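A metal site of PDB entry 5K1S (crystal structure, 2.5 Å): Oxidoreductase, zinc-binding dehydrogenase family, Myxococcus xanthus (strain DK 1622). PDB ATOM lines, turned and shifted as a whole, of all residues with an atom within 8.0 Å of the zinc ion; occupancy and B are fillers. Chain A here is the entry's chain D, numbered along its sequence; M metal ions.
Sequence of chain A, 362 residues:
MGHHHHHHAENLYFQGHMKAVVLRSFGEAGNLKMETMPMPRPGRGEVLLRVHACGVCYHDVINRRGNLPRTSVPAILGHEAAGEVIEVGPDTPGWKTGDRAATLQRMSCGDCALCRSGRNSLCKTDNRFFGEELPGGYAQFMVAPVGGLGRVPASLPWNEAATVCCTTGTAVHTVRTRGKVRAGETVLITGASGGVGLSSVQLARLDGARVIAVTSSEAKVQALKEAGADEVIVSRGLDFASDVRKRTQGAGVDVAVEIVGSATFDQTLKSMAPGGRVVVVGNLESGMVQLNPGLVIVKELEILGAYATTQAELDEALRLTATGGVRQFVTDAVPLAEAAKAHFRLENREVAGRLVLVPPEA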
ATOM      1  N   GLY A  55     -26.917 -24.865  -3.158  1.00  0.00           N
ATOM      2  CA  GLY A  55     -28.284 -24.433  -3.395  1.00  0.00           C
ATOM      3  C   GLY A  55     -29.208 -25.598  -3.677  1.00  0.00           C
ATOM      4  O   GLY A  55     -28.793 -26.669  -4.126  1.00  0.00           O
ATOM      5  N   VAL A  56     -30.494 -25.391  -3.407  1.00  0.00           N
ATOM      6  CA  VAL A  56     -31.512 -26.417  -3.571  1.00  0.00           C
ATOM      7  C   VAL A  56     -32.613 -25.844  -4.456  1.00  0.00           C
ATOM      8  O   VAL A  56     -33.197 -24.807  -4.129  1.00  0.00           O
ATOM      9  CB  VAL A  56     -32.093 -26.884  -2.226  1.00  0.00           C
ATOM     10  CG1 VAL A  56     -33.093 -28.017  -2.427  1.00  0.00           C
ATOM     11  CG2 VAL A  56     -30.973 -27.314  -1.291  1.00  0.00           C
ATOM     12  N   CYS A  57     -32.894 -26.516  -5.571  1.00  0.00           N
ATOM     13  CA  CYS A  57     -33.985 -26.144  -6.462  1.00  0.00           C
ATOM     14  C   CYS A  57     -34.813 -27.381  -6.775  1.00  0.00           C
ATOM     15  O   CYS A  57     -34.514 -28.490  -6.314  1.00  0.00           O
ATOM     16  CB  CYS A  57     -33.455 -25.493  -7.743  1.00  0.00           C
ATOM     17  SG  CYS A  57     -32.636 -26.634  -8.879  1.00  0.00           S
ATOM     18  N   TYR A  58     -35.862 -27.200  -7.578  1.00  0.00           N
ATOM     19  CA  TYR A  58     -36.802 -28.284  -7.836  1.00  0.00           C
ATOM     20  C   TYR A  58     -36.197 -29.391  -8.683  1.00  0.00           C
ATOM     21  O   TYR A  58     -36.716 -30.508  -8.686  1.00  0.00           O
ATOM     22  CB  TYR A  58     -38.056 -27.736  -8.523  1.00  0.00           C
ATOM     23  CG  TYR A  58     -39.271 -28.614  -8.354  1.00  0.00           C
ATOM     24  CD1 TYR A  58     -39.988 -28.623  -7.169  1.00  0.00           C
ATOM     25  CD2 TYR A  58     -39.705 -29.447  -9.383  1.00  0.00           C
ATOM     26  CE1 TYR A  58     -41.102 -29.429  -7.000  1.00  0.00           C
ATOM     27  CE2 TYR A  58     -40.815 -30.261  -9.228  1.00  0.00           C
ATOM     28  CZ  TYR A  58     -41.504 -30.243  -8.028  1.00  0.00           C
ATOM     29  OH  TYR A  58     -42.611 -31.040  -7.874  1.00  0.00           O
ATOM     30  N   HIS A  59     -35.102 -29.104  -9.403  1.00  0.00           N
ATOM     31  CA  HIS A  59     -34.476 -30.151 -10.209  1.00  0.00           C
ATOM     32  C   HIS A  59     -33.991 -31.313  -9.355  1.00  0.00           C
ATOM     33  O   HIS A  59     -34.011 -32.467  -9.796  1.00  0.00           O
ATOM     34  CB  HIS A  59     -33.308 -29.573 -11.006  1.00  0.00           C
ATOM     35  CG  HIS A  59     -32.594 -30.585 -11.850  1.00  0.00           C
ATOM     36  ND1 HIS A  59     -33.207 -31.271 -12.871  1.00  0.00           N
ATOM     37  CD2 HIS A  59     -31.320 -31.039 -11.804  1.00  0.00           C
ATOM     38  CE1 HIS A  59     -32.339 -32.107 -13.422  1.00  0.00           C
ATOM     39  NE2 HIS A  59     -31.183 -31.982 -12.796  1.00  0.00           N
ATOM     40  N   ASP A  60     -33.557 -31.034  -8.124  1.00  0.00           N
ATOM     41  CA  ASP A  60     -33.140 -32.098  -7.225  1.00  0.00           C
ATOM     42  C   ASP A  60     -34.334 -32.896  -6.707  1.00  0.00           C
ATOM     43  O   ASP A  60     -34.203 -34.077  -6.401  1.00  0.00           O
ATOM     44  CB  ASP A  60     -32.346 -31.525  -6.057  1.00  0.00           C
ATOM     45  CG  ASP A  60     -30.998 -30.964  -6.471  1.00  0.00           C
ATOM     46  OD1 ASP A  60     -30.336 -31.587  -7.324  1.00  0.00           O
ATOM     47  OD2 ASP A  60     -30.614 -29.890  -5.964  1.00  0.00           O
ATOM     48  N   GLY A  78     -27.075 -33.016  -5.591  1.00  0.00           N
ATOM     49  CA  GLY A  78     -26.947 -31.570  -5.556  1.00  0.00           C
ATOM     50  C   GLY A  78     -25.983 -31.080  -6.609  1.00  0.00           C
ATOM     51  O   GLY A  78     -24.941 -31.689  -6.868  1.00  0.00           O
ATOM     52  N   HIS A  79     -26.326 -29.947  -7.238  1.00  0.00           N
ATOM     53  CA  HIS A  79     -25.495 -29.391  -8.306  1.00  0.00           C
ATOM     54  C   HIS A  79     -25.231 -27.901  -8.158  1.00  0.00           C
ATOM     55  O   HIS A  79     -24.374 -27.371  -8.883  1.00  0.00           O
ATOM     56  CB  HIS A  79     -26.129 -29.647  -9.681  1.00  0.00           C
ATOM     57  CG  HIS A  79     -27.473 -28.997  -9.876  1.00  0.00           C
ATOM     58  ND1 HIS A  79     -27.914 -28.587 -11.105  1.00  0.00           N
ATOM     59  CD2 HIS A  79     -28.460 -28.703  -8.997  1.00  0.00           C
ATOM     60  CE1 HIS A  79     -29.119 -28.061 -10.980  1.00  0.00           C
ATOM     61  NE2 HIS A  79     -29.475 -28.125  -9.716  1.00  0.00           N
ATOM     62  N   GLU A  80     -25.909 -27.198  -7.245  1.00  0.00           N
ATOM     63  CA  GLU A  80     -25.685 -25.766  -7.037  1.00  0.00           C
ATOM     64  C   GLU A  80     -24.654 -25.576  -5.917  1.00  0.00           C
ATOM     65  O   GLU A  80     -24.922 -25.039  -4.851  1.00  0.00           O
ATOM     66  CB  GLU A  80     -26.997 -25.065  -6.695  1.00  0.00           C
ATOM     67  CG  GLU A  80     -28.052 -25.155  -7.784  1.00  0.00           C
ATOM     68  CD  GLU A  80     -29.391 -24.558  -7.350  1.00  0.00           C
ATOM     69  OE1 GLU A  80     -29.397 -23.735  -6.412  1.00  0.00           O
ATOM     70  OE2 GLU A  80     -30.417 -24.923  -7.947  1.00  0.00           O
ATOM     71  N   ALA A  81     -23.435 -26.033  -6.207  1.00  0.00           N
ATOM     72  CA  ALA A  81     -22.381 -26.123  -5.204  1.00  0.00           C
ATOM     73  C   ALA A  81     -21.362 -25.002  -5.370  1.00  0.00           C
ATOM     74  O   ALA A  81     -21.037 -24.582  -6.480  1.00  0.00           O
ATOM     75  CB  ALA A  81     -21.676 -27.482  -5.279  1.00  0.00           C
ATOM     76  N   LEU A 104     -21.252 -26.054 -12.239  1.00  0.00           N
ATOM     77  CA  LEU A 104     -22.330 -26.004 -13.214  1.00  0.00           C
ATOM     78  C   LEU A 104     -23.435 -26.987 -12.816  1.00  0.00           C
ATOM     79  O   LEU A 104     -23.380 -27.631 -11.760  1.00  0.00           O
ATOM     80  CB  LEU A 104     -21.803 -26.328 -14.609  1.00  0.00           C
ATOM     81  CG  LEU A 104     -20.698 -25.446 -15.185  1.00  0.00           C
ATOM     82  CD1 LEU A 104     -20.209 -26.026 -16.503  1.00  0.00           C
ATOM     83  CD2 LEU A 104     -21.180 -24.015 -15.372  1.00  0.00           C
ATOM     84  N   GLN A 105     -24.434 -27.108 -13.674  1.00  0.00           N
ATOM     85  CA  GLN A 105     -25.419 -28.178 -13.539  1.00  0.00           C
ATOM     86  C   GLN A 105     -24.945 -29.458 -14.209  1.00  0.00           C
ATOM     87  O   GLN A 105     -25.141 -30.558 -13.681  1.00  0.00           O
ATOM     88  CB  GLN A 105     -26.765 -27.758 -14.130  1.00  0.00           C
ATOM     89  CG  GLN A 105     -27.378 -26.515 -13.507  1.00  0.00           C
ATOM     90  CD  GLN A 105     -27.290 -25.300 -14.394  1.00  0.00           C
ATOM     91  OE1 GLN A 105     -26.542 -25.274 -15.370  1.00  0.00           O
ATOM     92  NE2 GLN A 105     -28.062 -24.268 -14.060  1.00  0.00           N
ATOM     93  N   ALA A 162     -23.674 -19.871  -4.183  1.00  0.00           N
ATOM     94  CA  ALA A 162     -24.158 -21.218  -4.467  1.00  0.00           C
ATOM     95  C   ALA A 162     -25.414 -21.199  -5.333  1.00  0.00           C
ATOM     96  O   ALA A 162     -25.654 -22.139  -6.081  1.00  0.00           O
ATOM     97  CB  ALA A 162     -24.431 -21.954  -3.160  1.00  0.00           C
ATOM     98  N   THR A 163     -26.214 -20.135  -5.242  1.00  0.00           N
ATOM     99  CA  THR A 163     -27.503 -20.062  -5.921  1.00  0.00           C
ATOM    100  C   THR A 163     -27.447 -19.193  -7.184  1.00  0.00           C
ATOM    101  O   THR A 163     -28.478 -18.653  -7.610  1.00  0.00           O
ATOM    102  CB  THR A 163     -28.571 -19.529  -4.963  1.00  0.00           C
ATOM    103  OG1 THR A 163     -28.219 -18.211  -4.536  1.00  0.00           O
ATOM    104  CG2 THR A 163     -28.694 -20.434  -3.752  1.00  0.00           C
ATOM    105  N   CYS A 165     -25.692 -20.157 -10.369  1.00  0.00           N
ATOM    106  CA  CYS A 165     -25.666 -20.865 -11.643  1.00  0.00           C
ATOM    107  C   CYS A 165     -27.072 -21.223 -12.119  1.00  0.00           C
ATOM    108  O   CYS A 165     -27.356 -21.182 -13.328  1.00  0.00           O
ATOM    109  CB  CYS A 165     -24.807 -22.124 -11.541  1.00  0.00           C
ATOM    110  SG  CYS A 165     -24.605 -22.990 -13.101  1.00  0.00           S
ATOM    111  N   CYS A 166     -27.951 -21.575 -11.197  1.00  0.00           N
ATOM    112  CA  CYS A 166     -29.295 -22.007 -11.561  1.00  0.00           C
ATOM    113  C   CYS A 166     -30.298 -20.863 -11.682  1.00  0.00           C
ATOM    114  O   CYS A 166     -31.417 -21.088 -12.148  1.00  0.00           O
ATOM    115  CB  CYS A 166     -29.811 -23.036 -10.553  1.00  0.00           C
ATOM    116  SG  CYS A 166     -29.577 -24.736 -11.110  1.00  0.00           S
ATOM    117  N   THR A 167     -29.926 -19.651 -11.278  1.00  0.00           N
ATOM    118  CA  THR A 167     -30.773 -18.486 -11.474  1.00  0.00           C
ATOM    119  C   THR A 167     -30.160 -17.557 -12.503  1.00  0.00           C
ATOM    120  O   THR A 167     -30.568 -17.544 -13.662  1.00  0.00           O
ATOM    121  CB  THR A 167     -30.979 -17.722 -10.156  1.00  0.00           C
ATOM    122  OG1 THR A 167     -29.697 -17.382  -9.588  1.00  0.00           O
ATOM    123  CG2 THR A 167     -31.778 -18.538  -9.166  1.00  0.00           C
ATOM    124  N   THR A 170     -28.702 -19.301 -15.502  1.00  0.00           N
ATOM    125  CA  THR A 170     -29.713 -19.623 -16.499  1.00  0.00           C
ATOM    126  C   THR A 170     -30.141 -18.366 -17.262  1.00  0.00           C
ATOM    127  O   THR A 170     -30.367 -18.423 -18.471  1.00  0.00           O
ATOM    128  CB  THR A 170     -30.919 -20.272 -15.819  1.00  0.00           C
ATOM    129  OG1 THR A 170     -30.501 -21.474 -15.168  1.00  0.00           O
ATOM    130  CG2 THR A 170     -32.004 -20.609 -16.848  1.00  0.00           C
ATOM    131  N   ARG A 354     -34.463 -18.862  -2.585  1.00  0.00           N
ATOM    132  CA  ARG A 354     -33.583 -20.003  -2.841  1.00  0.00           C
ATOM    133  C   ARG A 354     -33.094 -20.599  -1.517  1.00  0.00           C
ATOM    134  O   ARG A 354     -32.771 -19.858  -0.579  1.00  0.00           O
ATOM    135  CB  ARG A 354     -32.378 -19.584  -3.695  1.00  0.00           C
ATOM    136  CG  ARG A 354     -32.575 -19.804  -5.190  1.00  0.00           C
ATOM    137  CD  ARG A 354     -32.593 -21.289  -5.540  1.00  0.00           C
ATOM    138  NE  ARG A 354     -32.819 -21.515  -6.965  1.00  0.00           N
ATOM    139  CZ  ARG A 354     -34.000 -21.397  -7.557  1.00  0.00           C
ATOM    140  NH1 ARG A 354     -35.069 -21.044  -6.857  1.00  0.00           N
ATOM    141  NH2 ARG A 354     -34.116 -21.634  -8.862  1.00  0.00           N
HETATM  142 ZN    ZN M   1     -30.506 -26.283  -9.667  1.00  0.00          ZN
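The backbone carbonyl oxygen (O) of Glu 80 lies within hydrogen-bond range of the backbone NH (N) of Gly 55.
The backbone NH (N) of His 59 sits close to the side-chain sulfur (SG) of Cys 57, at 3.5 Å.
The side-chain sulfur (SG) of Cys 166 lies close to the side-chain amide nitrogen (NE2) of Gln 105.
O of Cys 166 lies within hydrogen-bond range of OG1 of Thr 170, at 3.2 Å.
Four residues have an atom within 4 Å of the zinc ion: Cys 57, His 79, Glu 80 and Cys 166.
Along chain A the residues within 4 Å of the zinc ion span positions 57 to 166.
The zinc ion is bound by NE2 of His 79, OE2 of Glu 80, SG of Cys 57 and SG of Cys 166.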
